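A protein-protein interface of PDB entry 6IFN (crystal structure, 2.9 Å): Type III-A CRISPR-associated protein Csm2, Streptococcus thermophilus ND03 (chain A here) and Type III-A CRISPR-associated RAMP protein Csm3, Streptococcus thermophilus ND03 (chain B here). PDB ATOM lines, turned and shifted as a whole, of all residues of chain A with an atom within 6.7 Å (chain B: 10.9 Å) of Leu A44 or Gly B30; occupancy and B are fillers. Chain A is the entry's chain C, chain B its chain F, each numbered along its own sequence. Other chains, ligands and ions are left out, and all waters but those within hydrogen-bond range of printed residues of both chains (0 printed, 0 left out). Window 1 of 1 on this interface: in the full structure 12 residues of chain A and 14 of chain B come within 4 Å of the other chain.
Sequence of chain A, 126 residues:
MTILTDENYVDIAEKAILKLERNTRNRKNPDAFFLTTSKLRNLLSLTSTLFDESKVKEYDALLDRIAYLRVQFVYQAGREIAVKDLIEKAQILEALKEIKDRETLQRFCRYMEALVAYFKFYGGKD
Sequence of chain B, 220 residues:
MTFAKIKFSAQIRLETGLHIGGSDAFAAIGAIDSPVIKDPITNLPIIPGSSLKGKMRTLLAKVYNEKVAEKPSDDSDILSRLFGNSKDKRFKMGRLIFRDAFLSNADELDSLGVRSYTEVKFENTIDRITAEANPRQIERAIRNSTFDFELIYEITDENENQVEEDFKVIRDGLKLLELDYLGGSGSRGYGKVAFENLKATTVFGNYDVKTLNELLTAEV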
ATOM      1  N   THR A  37      -7.836   7.438 -10.971  1.00  0.00           N
ATOM      2  CA  THR A  37      -6.591   7.250 -11.704  1.00  0.00           C
ATOM      3  C   THR A  37      -5.470   8.045 -11.034  1.00  0.00           C
ATOM      4  O   THR A  37      -4.349   7.567 -10.963  1.00  0.00           O
ATOM      5  CB  THR A  37      -6.751   7.635 -13.178  1.00  0.00           C
ATOM      6  OG1 THR A  37      -7.966   7.077 -13.680  1.00  0.00           O
ATOM      7  CG2 THR A  37      -5.595   7.150 -14.024  1.00  0.00           C
ATOM      8  N   LYS A  39      -4.894   8.455  -7.969  1.00  0.00           N
ATOM      9  CA  LYS A  39      -4.335   7.684  -6.851  1.00  0.00           C
ATOM     10  C   LYS A  39      -3.303   6.671  -7.371  1.00  0.00           C
ATOM     11  O   LYS A  39      -2.243   6.491  -6.770  1.00  0.00           O
ATOM     12  CB  LYS A  39      -5.447   7.005  -6.052  1.00  0.00           C
ATOM     13  CG  LYS A  39      -6.415   7.961  -5.354  1.00  0.00           C
ATOM     14  CD  LYS A  39      -7.774   7.337  -4.992  1.00  0.00           C
ATOM     15  CE  LYS A  39      -8.852   8.314  -4.563  1.00  0.00           C
ATOM     16  NZ  LYS A  39      -8.298   9.530  -3.923  1.00  0.00           N
ATOM     17  N   LEU A  40      -3.590   6.049  -8.517  1.00  0.00           N
ATOM     18  CA  LEU A  40      -2.707   5.038  -9.093  1.00  0.00           C
ATOM     19  C   LEU A  40      -1.498   5.651  -9.830  1.00  0.00           C
ATOM     20  O   LEU A  40      -0.562   4.918 -10.120  1.00  0.00           O
ATOM     21  CB  LEU A  40      -3.517   4.172 -10.062  1.00  0.00           C
ATOM     22  CG  LEU A  40      -4.666   3.384  -9.446  1.00  0.00           C
ATOM     23  CD1 LEU A  40      -5.172   2.312 -10.394  1.00  0.00           C
ATOM     24  CD2 LEU A  40      -4.238   2.772  -8.125  1.00  0.00           C
ATOM     25  N   ARG A  41      -1.525   6.938 -10.202  1.00  0.00           N
ATOM     26  CA  ARG A  41      -0.603   7.445 -11.237  1.00  0.00           C
ATOM     27  C   ARG A  41       0.859   7.136 -10.885  1.00  0.00           C
ATOM     28  O   ARG A  41       1.571   6.517 -11.658  1.00  0.00           O
ATOM     29  CB  ARG A  41      -0.821   8.934 -11.533  1.00  0.00           C
ATOM     30  CG  ARG A  41      -0.419   9.899 -10.429  1.00  0.00           C
ATOM     31  CD  ARG A  41      -0.675  11.334 -10.838  1.00  0.00           C
ATOM     32  NE  ARG A  41      -0.048  11.601 -12.131  1.00  0.00           N
ATOM     33  CZ  ARG A  41      -0.697  11.937 -13.242  1.00  0.00           C
ATOM     34  NH1 ARG A  41      -2.021  11.932 -13.262  1.00  0.00           N
ATOM     35  NH2 ARG A  41      -0.015  12.310 -14.318  1.00  0.00           N
ATOM     36  N   ASN A  42       1.308   7.568  -9.716  1.00  0.00           N
ATOM     37  CA  ASN A  42       2.698   7.431  -9.339  1.00  0.00           C
ATOM     38  C   ASN A  42       3.073   5.950  -9.206  1.00  0.00           C
ATOM     39  O   ASN A  42       4.216   5.614  -9.263  1.00  0.00           O
ATOM     40  CB  ASN A  42       3.009   8.206  -8.051  1.00  0.00           C
ATOM     41  CG  ASN A  42       2.400   7.606  -6.793  1.00  0.00           C
ATOM     42  OD1 ASN A  42       2.964   6.674  -6.217  1.00  0.00           O
ATOM     43  ND2 ASN A  42       1.281   8.160  -6.335  1.00  0.00           N
ATOM     44  N   LEU A  43       2.096   5.078  -8.968  1.00  0.00           N
ATOM     45  CA  LEU A  43       2.298   3.655  -8.772  1.00  0.00           C
ATOM     46  C   LEU A  43       2.549   3.002 -10.125  1.00  0.00           C
ATOM     47  O   LEU A  43       3.541   2.300 -10.317  1.00  0.00           O
ATOM     48  CB  LEU A  43       1.014   3.099  -8.140  1.00  0.00           C
ATOM     49  CG  LEU A  43       1.079   1.776  -7.384  1.00  0.00           C
ATOM     50  CD1 LEU A  43       2.124   1.809  -6.278  1.00  0.00           C
ATOM     51  CD2 LEU A  43      -0.288   1.468  -6.803  1.00  0.00           C
ATOM     52  N   LEU A  44       1.620   3.208 -11.059  1.00  0.00           N
ATOM     53  CA  LEU A  44       1.698   2.492 -12.335  1.00  0.00           C
ATOM     54  C   LEU A  44       2.714   3.163 -13.274  1.00  0.00           C
ATOM     55  O   LEU A  44       3.197   2.531 -14.189  1.00  0.00           O
ATOM     56  CB  LEU A  44       0.311   2.279 -12.959  1.00  0.00           C
ATOM     57  CG  LEU A  44      -0.622   3.471 -13.070  1.00  0.00           C
ATOM     58  CD1 LEU A  44      -0.024   4.538 -13.977  1.00  0.00           C
ATOM     59  CD2 LEU A  44      -1.979   3.014 -13.579  1.00  0.00           C
ATOM     60  N   SER A  45       3.114   4.400 -13.001  1.00  0.00           N
ATOM     61  CA  SER A  45       4.337   4.945 -13.588  1.00  0.00           C
ATOM     62  C   SER A  45       5.525   4.026 -13.247  1.00  0.00           C
ATOM     63  O   SER A  45       6.310   3.675 -14.099  1.00  0.00           O
ATOM     64  CB  SER A  45       4.537   6.382 -13.146  1.00  0.00           C
ATOM     65  OG  SER A  45       5.899   6.749 -13.067  1.00  0.00           O
ATOM     66  N   LEU A  46       5.651   3.625 -11.985  1.00  0.00           N
ATOM     67  CA  LEU A  46       6.757   2.743 -11.580  1.00  0.00           C
ATOM     68  C   LEU A  46       6.636   1.383 -12.289  1.00  0.00           C
ATOM     69  O   LEU A  46       7.640   0.866 -12.805  1.00  0.00           O
ATOM     70  CB  LEU A  46       6.771   2.564 -10.058  1.00  0.00           C
ATOM     71  CG  LEU A  46       7.095   3.813  -9.231  1.00  0.00           C
ATOM     72  CD1 LEU A  46       6.399   3.754  -7.869  1.00  0.00           C
ATOM     73  CD2 LEU A  46       8.601   4.008  -9.064  1.00  0.00           C
ATOM     74  N   THR A  47       5.422   0.817 -12.342  1.00  0.00           N
ATOM     75  CA  THR A  47       5.187  -0.442 -13.073  1.00  0.00           C
ATOM     76  C   THR A  47       5.713  -0.335 -14.514  1.00  0.00           C
ATOM     77  O   THR A  47       6.429  -1.208 -14.980  1.00  0.00           O
ATOM     78  CB  THR A  47       3.698  -0.805 -13.072  1.00  0.00           C
ATOM     79  OG1 THR A  47       3.422  -1.517 -11.868  1.00  0.00           O
ATOM     80  CG2 THR A  47       3.292  -1.632 -14.271  1.00  0.00           C
ATOM     81  N   SER A  48       5.338   0.743 -15.209  1.00  0.00           N
ATOM     82  CA  SER A  48       5.718   0.949 -16.594  1.00  0.00           C
ATOM     83  C   SER A  48       7.234   1.102 -16.719  1.00  0.00           C
ATOM     84  O   SER A  48       7.811   0.500 -17.606  1.00  0.00           O
ATOM     85  CB  SER A  48       4.970   2.101 -17.207  1.00  0.00           C
ATOM     86  OG  SER A  48       3.580   1.794 -17.249  1.00  0.00           O
ATOM     87  N   THR A  49       7.877   1.853 -15.816  1.00  0.00           N
ATOM     88  CA  THR A  49       9.343   1.979 -15.879  1.00  0.00           C
ATOM     89  C   THR A  49       9.999   0.601 -15.705  1.00  0.00           C
ATOM     90  O   THR A  49      11.048   0.342 -16.297  1.00  0.00           O
ATOM     91  CB  THR A  49       9.929   2.953 -14.852  1.00  0.00           C
ATOM     92  OG1 THR A  49       9.104   4.117 -14.799  1.00  0.00           O
ATOM     93  CG2 THR A  49      11.360   3.338 -15.184  1.00  0.00           C
ATOM     94  N   LEU A  69       8.711  -1.185  -5.805  1.00  0.00           N
ATOM     95  CA  LEU A  69       7.315  -1.347  -6.255  1.00  0.00           C
ATOM     96  C   LEU A  69       6.435  -1.813  -5.079  1.00  0.00           C
ATOM     97  O   LEU A  69       5.443  -1.174  -4.744  1.00  0.00           O
ATOM     98  CB  LEU A  69       7.236  -2.353  -7.417  1.00  0.00           C
ATOM     99  CG  LEU A  69       6.357  -1.962  -8.614  1.00  0.00           C
ATOM    100  CD1 LEU A  69       5.810  -3.185  -9.326  1.00  0.00           C
ATOM    101  CD2 LEU A  69       5.208  -1.040  -8.224  1.00  0.00           C
ATOM    102  N   PHE A  73       3.274   0.108  -3.302  1.00  0.00           N
ATOM    103  CA  PHE A  73       1.953  -0.487  -3.345  1.00  0.00           C
ATOM    104  C   PHE A  73       1.316  -0.453  -1.958  1.00  0.00           C
ATOM    105  O   PHE A  73       0.251   0.159  -1.788  1.00  0.00           O
ATOM    106  CB  PHE A  73       1.983  -1.908  -3.912  1.00  0.00           C
ATOM    107  CG  PHE A  73       1.567  -1.980  -5.363  1.00  0.00           C
ATOM    108  CD1 PHE A  73       0.236  -1.849  -5.727  1.00  0.00           C
ATOM    109  CD2 PHE A  73       2.512  -2.143  -6.365  1.00  0.00           C
ATOM    110  CE1 PHE A  73      -0.132  -1.885  -7.062  1.00  0.00           C
ATOM    111  CE2 PHE A  73       2.140  -2.197  -7.699  1.00  0.00           C
ATOM    112  CZ  PHE A  73       0.819  -2.064  -8.042  1.00  0.00           C
ATOM    113  N   MET A 112      -1.309  -4.952 -14.728  1.00  0.00           N
ATOM    114  CA  MET A 112      -1.701  -3.638 -14.281  1.00  0.00           C
ATOM    115  C   MET A 112      -2.392  -2.904 -15.441  1.00  0.00           C
ATOM    116  O   MET A 112      -3.443  -2.324 -15.238  1.00  0.00           O
ATOM    117  CB  MET A 112      -0.500  -2.840 -13.765  1.00  0.00           C
ATOM    118  CG  MET A 112       0.104  -3.426 -12.493  1.00  0.00           C
ATOM    119  SD  MET A 112      -1.117  -3.717 -11.187  1.00  0.00           S
ATOM    120  CE  MET A 112      -1.720  -2.039 -10.993  1.00  0.00           C
ATOM    121  N   GLU A 113      -1.795  -2.960 -16.642  1.00  0.00           N
ATOM    122  CA  GLU A 113      -2.316  -2.300 -17.832  1.00  0.00           C
ATOM    123  C   GLU A 113      -3.773  -2.711 -17.978  1.00  0.00           C
ATOM    124  O   GLU A 113      -4.629  -1.872 -18.189  1.00  0.00           O
ATOM    125  CB  GLU A 113      -1.563  -2.686 -19.113  1.00  0.00           C
ATOM    126  CG  GLU A 113      -0.254  -1.940 -19.369  1.00  0.00           C
ATOM    127  CD  GLU A 113       0.216  -1.963 -20.827  1.00  0.00           C
ATOM    128  OE1 GLU A 113       1.458  -1.764 -21.067  1.00  0.00           O
ATOM    129  OE2 GLU A 113      -0.663  -2.163 -21.732  1.00  0.00           O
ATOM    130  N   VAL A 116      -6.271  -1.315 -15.383  1.00  0.00           N
ATOM    131  CA  VAL A 116      -6.506   0.117 -15.562  1.00  0.00           C
ATOM    132  C   VAL A 116      -7.448   0.317 -16.750  1.00  0.00           C
ATOM    133  O   VAL A 116      -8.350   1.136 -16.687  1.00  0.00           O
ATOM    134  CB  VAL A 116      -5.190   0.892 -15.764  1.00  0.00           C
ATOM    135  CG1 VAL A 116      -5.412   2.355 -16.116  1.00  0.00           C
ATOM    136  CG2 VAL A 116      -4.276   0.780 -14.552  1.00  0.00           C
ATOM    137  N   LYS A 120     -11.112   2.189 -16.399  1.00  0.00           N
ATOM    138  CA  LYS A 120     -11.574   3.333 -17.153  1.00  0.00           C
ATOM    139  C   LYS A 120     -12.817   2.946 -17.974  1.00  0.00           C
ATOM    140  O   LYS A 120     -13.729   3.753 -18.167  1.00  0.00           O
ATOM    141  CB  LYS A 120     -10.446   3.868 -18.041  1.00  0.00           C
ATOM    142  CG  LYS A 120      -9.621   4.983 -17.421  1.00  0.00           C
ATOM    143  CD  LYS A 120     -10.267   6.353 -17.579  1.00  0.00           C
ATOM    144  CE  LYS A 120      -9.367   7.512 -17.188  1.00  0.00           C
ATOM    145  NZ  LYS A 120     -10.141   8.767 -17.017  1.00  0.00           N
ATOM    146  N   SER B  23       2.722  11.450 -29.659  1.00  0.00           N
ATOM    147  CA  SER B  23       1.854  10.349 -30.030  1.00  0.00           C
ATOM    148  C   SER B  23       0.841  10.154 -28.906  1.00  0.00           C
ATOM    149  O   SER B  23       1.169   9.505 -27.912  1.00  0.00           O
ATOM    150  CB  SER B  23       2.654   9.101 -30.299  1.00  0.00           C
ATOM    151  N   ASP B  24      -0.367  10.718 -29.061  1.00  0.00           N
ATOM    152  CA  ASP B  24      -1.392  10.690 -27.974  1.00  0.00           C
ATOM    153  C   ASP B  24      -2.154   9.354 -27.977  1.00  0.00           C
ATOM    154  O   ASP B  24      -2.336   8.761 -26.949  1.00  0.00           O
ATOM    155  CB  ASP B  24      -2.337  11.894 -28.032  1.00  0.00           C
ATOM    156  CG  ASP B  24      -2.612  12.502 -26.661  1.00  0.00           C
ATOM    157  OD1 ASP B  24      -2.573  11.748 -25.659  1.00  0.00           O
ATOM    158  OD2 ASP B  24      -2.826  13.737 -26.594  1.00  0.00           O
ATOM    159  N   ALA B  25      -2.648   8.922 -29.139  1.00  0.00           N
ATOM    160  CA  ALA B  25      -3.385   7.671 -29.280  1.00  0.00           C
ATOM    161  C   ALA B  25      -2.449   6.457 -29.301  1.00  0.00           C
ATOM    162  O   ALA B  25      -2.940   5.357 -29.352  1.00  0.00           O
ATOM    163  CB  ALA B  25      -4.222   7.692 -30.534  1.00  0.00           C
ATOM    164  N   PHE B  26      -1.126   6.652 -29.366  1.00  0.00           N
ATOM    165  CA  PHE B  26      -0.161   5.558 -29.230  1.00  0.00           C
ATOM    166  C   PHE B  26       0.480   5.597 -27.847  1.00  0.00           C
ATOM    167  O   PHE B  26       1.447   4.886 -27.583  1.00  0.00           O
ATOM    168  CB  PHE B  26       0.894   5.616 -30.336  1.00  0.00           C
ATOM    169  CG  PHE B  26       0.307   5.202 -31.654  1.00  0.00           C
ATOM    170  CD1 PHE B  26      -0.371   6.123 -32.438  1.00  0.00           C
ATOM    171  CD2 PHE B  26       0.329   3.876 -32.047  1.00  0.00           C
ATOM    172  CE1 PHE B  26      -0.971   5.734 -33.627  1.00  0.00           C
ATOM    173  CE2 PHE B  26      -0.267   3.493 -33.239  1.00  0.00           C
ATOM    174  CZ  PHE B  26      -0.924   4.420 -34.022  1.00  0.00           C
ATOM    175  N   ALA B  27      -0.096   6.407 -26.954  1.00  0.00           N
ATOM    176  CA  ALA B  27       0.449   6.635 -25.604  1.00  0.00           C
ATOM    177  C   ALA B  27       0.391   5.347 -24.768  1.00  0.00           C
ATOM    178  O   ALA B  27      -0.361   4.435 -25.079  1.00  0.00           O
ATOM    179  CB  ALA B  27      -0.320   7.739 -24.934  1.00  0.00           C
ATOM    180  N   ALA B  28       1.208   5.308 -23.707  1.00  0.00           N
ATOM    181  CA  ALA B  28       1.084   4.361 -22.587  1.00  0.00           C
ATOM    182  C   ALA B  28      -0.340   4.422 -22.014  1.00  0.00           C
ATOM    183  O   ALA B  28      -0.931   5.491 -21.942  1.00  0.00           O
ATOM    184  CB  ALA B  28       2.106   4.704 -21.531  1.00  0.00           C
ATOM    185  N   ILE B  29      -0.869   3.258 -21.615  1.00  0.00           N
ATOM    186  CA  ILE B  29      -2.212   3.140 -21.049  1.00  0.00           C
ATOM    187  C   ILE B  29      -2.243   3.802 -19.658  1.00  0.00           C
ATOM    188  O   ILE B  29      -3.331   4.072 -19.122  1.00  0.00           O
ATOM    189  CB  ILE B  29      -2.666   1.661 -21.052  1.00  0.00           C
ATOM    190  CG1 ILE B  29      -3.279   1.290 -22.409  1.00  0.00           C
ATOM    191  CG2 ILE B  29      -3.606   1.333 -19.895  1.00  0.00           C
ATOM    192  CD1 ILE B  29      -3.267  -0.187 -22.709  1.00  0.00           C
ATOM    193  N   GLY B  30      -1.051   4.020 -19.115  1.00  0.00           N
ATOM    194  CA  GLY B  30      -0.860   4.659 -17.806  1.00  0.00           C
ATOM    195  C   GLY B  30      -1.960   5.630 -17.440  1.00  0.00           C
ATOM    196  O   GLY B  30      -3.110   5.229 -17.394  1.00  0.00           O
ATOM    197  N   ALA B  31      -1.584   6.893 -17.265  1.00  0.00           N
ATOM    198  CA  ALA B  31      -2.491   7.958 -16.788  1.00  0.00           C
ATOM    199  C   ALA B  31      -2.366   9.180 -17.688  1.00  0.00           C
ATOM    200  O   ALA B  31      -1.728   9.074 -18.742  1.00  0.00           O
ATOM    201  CB  ALA B  31      -2.131   8.308 -15.371  1.00  0.00           C
ATOM    202  N   ILE B  32      -3.016  10.275 -17.298  1.00  0.00           N
ATOM    203  CA  ILE B  32      -2.945  11.519 -18.104  1.00  0.00           C
ATOM    204  C   ILE B  32      -1.502  11.996 -18.121  1.00  0.00           C
ATOM    205  O   ILE B  32      -0.850  11.957 -17.086  1.00  0.00           O
ATOM    206  CB  ILE B  32      -3.818  12.626 -17.506  1.00  0.00           C
ATOM    207  CG1 ILE B  32      -4.903  12.081 -16.589  1.00  0.00           C
ATOM    208  CG2 ILE B  32      -4.378  13.509 -18.600  1.00  0.00           C
ATOM    209  CD1 ILE B  32      -5.473  13.135 -15.686  1.00  0.00           C
ATOM    210  N   ASP B  33      -1.037  12.379 -19.294  1.00  0.00           N
ATOM    211  CA  ASP B  33       0.297  12.986 -19.495  1.00  0.00           C
ATOM    212  C   ASP B  33       0.323  13.500 -20.920  1.00  0.00           C
ATOM    213  O   ASP B  33      -0.387  12.928 -21.760  1.00  0.00           O
ATOM    214  CB  ASP B  33       1.364  11.905 -19.605  1.00  0.00           C
ATOM    215  CG  ASP B  33       2.202  11.721 -18.367  1.00  0.00           C
ATOM    216  OD1 ASP B  33       2.362  12.688 -17.655  1.00  0.00           O
ATOM    217  OD2 ASP B  33       2.677  10.612 -18.142  1.00  0.00           O
ATOM    218  N   SER B  34       1.126  14.504 -21.216  1.00  0.00           N
ATOM    219  CA  SER B  34       1.302  14.730 -22.663  1.00  0.00           C
ATOM    220  C   SER B  34       2.602  13.969 -22.894  1.00  0.00           C
ATOM    221  O   SER B  34       3.621  14.428 -22.419  1.00  0.00           O
ATOM    222  CB  SER B  34       1.349  16.173 -23.009  1.00  0.00           C
ATOM    223  OG  SER B  34       2.475  16.779 -22.436  1.00  0.00           O
ATOM    224  N   PRO B  35       2.594  12.793 -23.547  1.00  0.00           N
ATOM    225  CA  PRO B  35       3.768  11.935 -23.617  1.00  0.00           C
ATOM    226  C   PRO B  35       4.913  12.486 -24.456  1.00  0.00           C
ATOM    227  O   PRO B  35       4.664  13.307 -25.268  1.00  0.00           O
ATOM    228  CB  PRO B  35       3.240  10.673 -24.291  1.00  0.00           C
ATOM    229  CG  PRO B  35       2.121  11.172 -25.138  1.00  0.00           C
ATOM    230  CD  PRO B  35       1.475  12.234 -24.284  1.00  0.00           C
ATOM    231  N   LYS B  38       9.611   8.528 -27.698  1.00  0.00           N
ATOM    232  CA  LYS B  38      10.453   7.510 -27.061  1.00  0.00           C
ATOM    233  C   LYS B  38      10.896   6.461 -28.081  1.00  0.00           C
ATOM    234  O   LYS B  38      10.161   6.109 -28.968  1.00  0.00           O
ATOM    235  CB  LYS B  38       9.725   6.829 -25.899  1.00  0.00           C
ATOM    236  CG  LYS B  38       9.180   7.777 -24.841  1.00  0.00           C
ATOM    237  CD  LYS B  38       8.633   7.105 -23.602  1.00  0.00           C
ATOM    238  CE  LYS B  38       8.204   8.102 -22.534  1.00  0.00           C
ATOM    239  NZ  LYS B  38       6.866   8.655 -22.811  1.00  0.00           N
ATOM    240  N   ASN B  43      12.038   2.231 -24.646  1.00  0.00           N
ATOM    241  CA  ASN B  43      11.039   3.141 -24.086  1.00  0.00           C
ATOM    242  C   ASN B  43      11.713   4.349 -23.414  1.00  0.00           C
ATOM    243  O   ASN B  43      11.089   4.994 -22.595  1.00  0.00           O
ATOM    244  CB  ASN B  43      10.116   2.378 -23.129  1.00  0.00           C
ATOM    245  CG  ASN B  43       8.773   3.032 -22.894  1.00  0.00           C
ATOM    246  OD1 ASN B  43       8.353   3.926 -23.639  1.00  0.00           O
ATOM    247  ND2 ASN B  43       8.070   2.540 -21.878  1.00  0.00           N
ATOM    248  N   ARG B 115      14.535   6.801 -10.461  1.00  0.00           N
ATOM    249  CA  ARG B 115      13.540   5.713 -10.525  1.00  0.00           C
ATOM    250  C   ARG B 115      12.693   5.865 -11.798  1.00  0.00           C
ATOM    251  O   ARG B 115      11.785   5.086 -12.036  1.00  0.00           O
ATOM    252  CB  ARG B 115      12.687   5.686  -9.249  1.00  0.00           C
ATOM    253  CG  ARG B 115      13.475   5.317  -7.995  1.00  0.00           C
ATOM    254  CD  ARG B 115      12.711   5.502  -6.698  1.00  0.00           C
ATOM    255  NE  ARG B 115      12.865   6.818  -6.090  1.00  0.00           N
ATOM    256  CZ  ARG B 115      12.462   7.134  -4.863  1.00  0.00           C
ATOM    257  NH1 ARG B 115      11.990   6.194  -4.062  1.00  0.00           N
ATOM    258  NH2 ARG B 115      12.536   8.385  -4.437  1.00  0.00           N
ATOM    259  N   SER B 116      13.012   6.874 -12.610  1.00  0.00           N
ATOM    260  CA  SER B 116      12.372   7.098 -13.897  1.00  0.00           C
ATOM    261  C   SER B 116      13.231   8.071 -14.699  1.00  0.00           C
ATOM    262  O   SER B 116      13.981   8.848 -14.108  1.00  0.00           O
ATOM    263  CB  SER B 116      10.979   7.623 -13.758  1.00  0.00           C
ATOM    264  OG  SER B 116      10.562   8.168 -14.997  1.00  0.00           O
ATOM    265  N   THR B 118      11.780  10.113 -16.913  1.00  0.00           N
ATOM    266  CA  THR B 118      10.884  11.213 -17.214  1.00  0.00           C
ATOM    267  C   THR B 118      10.125  11.613 -15.946  1.00  0.00           C
ATOM    268  O   THR B 118       9.662  10.762 -15.192  1.00  0.00           O
ATOM    269  CB  THR B 118       9.904  10.855 -18.340  1.00  0.00           C
ATOM    270  OG1 THR B 118       9.139   9.729 -17.923  1.00  0.00           O
ATOM    271  CG2 THR B 118      10.599  10.535 -19.646  1.00  0.00           C
ATOM    272  N   VAL B 120       6.862  14.008 -14.452  1.00  0.00           N
ATOM    273  CA  VAL B 120       5.605  14.626 -14.783  1.00  0.00           C
ATOM    274  C   VAL B 120       5.552  16.002 -14.119  1.00  0.00           C
ATOM    275  O   VAL B 120       5.523  16.091 -12.891  1.00  0.00           O
ATOM    276  CB  VAL B 120       4.429  13.777 -14.280  1.00  0.00           C
ATOM    277  CG1 VAL B 120       3.123  14.263 -14.877  1.00  0.00           C
ATOM    278  CG2 VAL B 120       4.642  12.288 -14.514  1.00  0.00           C
ATOM    279  N   GLN B 137      -1.027  18.214 -16.394  1.00  0.00           N
ATOM    280  CA  GLN B 137       0.221  17.457 -16.201  1.00  0.00           C
ATOM    281  C   GLN B 137       0.870  17.274 -17.581  1.00  0.00           C
ATOM    282  O   GLN B 137       0.151  17.045 -18.578  1.00  0.00           O
ATOM    283  CB  GLN B 137      -0.025  16.075 -15.583  1.00  0.00           C
ATOM    284  CG  GLN B 137      -1.029  16.042 -14.450  1.00  0.00           C
ATOM    285  CD  GLN B 137      -2.439  16.087 -14.982  1.00  0.00           C
ATOM    286  OE1 GLN B 137      -2.855  15.198 -15.717  1.00  0.00           O
ATOM    287  NE2 GLN B 137      -3.182  17.133 -14.640  1.00  0.00           N
ATOM    288  N   GLU B 139       4.649  15.661 -19.500  1.00  0.00           N
ATOM    289  CA  GLU B 139       5.820  14.815 -19.309  1.00  0.00           C
ATOM    290  C   GLU B 139       7.050  15.549 -19.844  1.00  0.00           C
ATOM    291  O   GLU B 139       6.971  16.193 -20.884  1.00  0.00           O
ATOM    292  CB  GLU B 139       5.647  13.468 -20.011  1.00  0.00           C
ATOM    293  CG  GLU B 139       6.772  12.454 -19.758  1.00  0.00           C
ATOM    294  CD  GLU B 139       6.509  10.995 -20.186  1.00  0.00           C
ATOM    295  OE1 GLU B 139       5.488  10.720 -20.887  1.00  0.00           O
ATOM    296  OE2 GLU B 139       7.322  10.104 -19.828  1.00  0.00           O
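Among the printed residues, merely in contact across the chains: Glu A113 with Ile B29 (3.4 Å), Thr A49 with Arg B115 (3.6 Å), Arg A41 with Val B120 (3.7 Å), Arg A41 with Gln B137 (3.9 Å), Thr A37 with Ala B31 (3.9 Å), Val A116 with Gly B30 (3.9 Å) and Leu A44 with Gly B30 (3.9 Å).
O of Ile B32 lies within hydrogen-bond range of NH2 of Arg A41 (2.9 Å).
Leu A44 touches just one residue of chain B: Gly B30.
No residue of chain B comes within 4 Å of Leu A40.
No residue of chain B comes within 4 Å of Leu A43.
No residue of chain B comes within 4 Å of Ser A45.
No residue of chain B comes within 4 Å of Thr A47.
Ser A48 touches none of the printed residues of chain B.
Printed residues of chain A within 4 Å of Arg B115: Thr A49.
Printed residues of chain B within 4 Å of Thr A49: Arg B115 (3.6 Å).
Of the printed residues of chain B, Thr A37 touches Ala B31.
Ala B27 touches none of the printed residues of chain A.
The nearest residue of chain B that does not touch Leu A44 is Ala B31 (4.3 Å).
The nearest residue of chain A that does not touch Gly B30 is Thr A37 (4.6 Å).
Of the 18 printed residues of chain A, 6 touch a printed residue of chain B.
Hydrophobic or aromatic side chains of chain A that line the printed part of chain B: Leu A44 and Val A116.
Among the printed residues, 8 pairs touch across the chains.
Among the printed residues, no Asp or Glu carboxylate lies within 4 Å of a Lys or Arg side-chain nitrogen of the other chain.
O of Leu A44 is in hydrogen-bond range of OG of Ser A48, at 3.2 Å.
The backbone carbonyl oxygen (O) of Ser A45 lies within hydrogen-bond range of the side-chain hydroxyl (OG1) of Thr A49 (2.9 Å).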
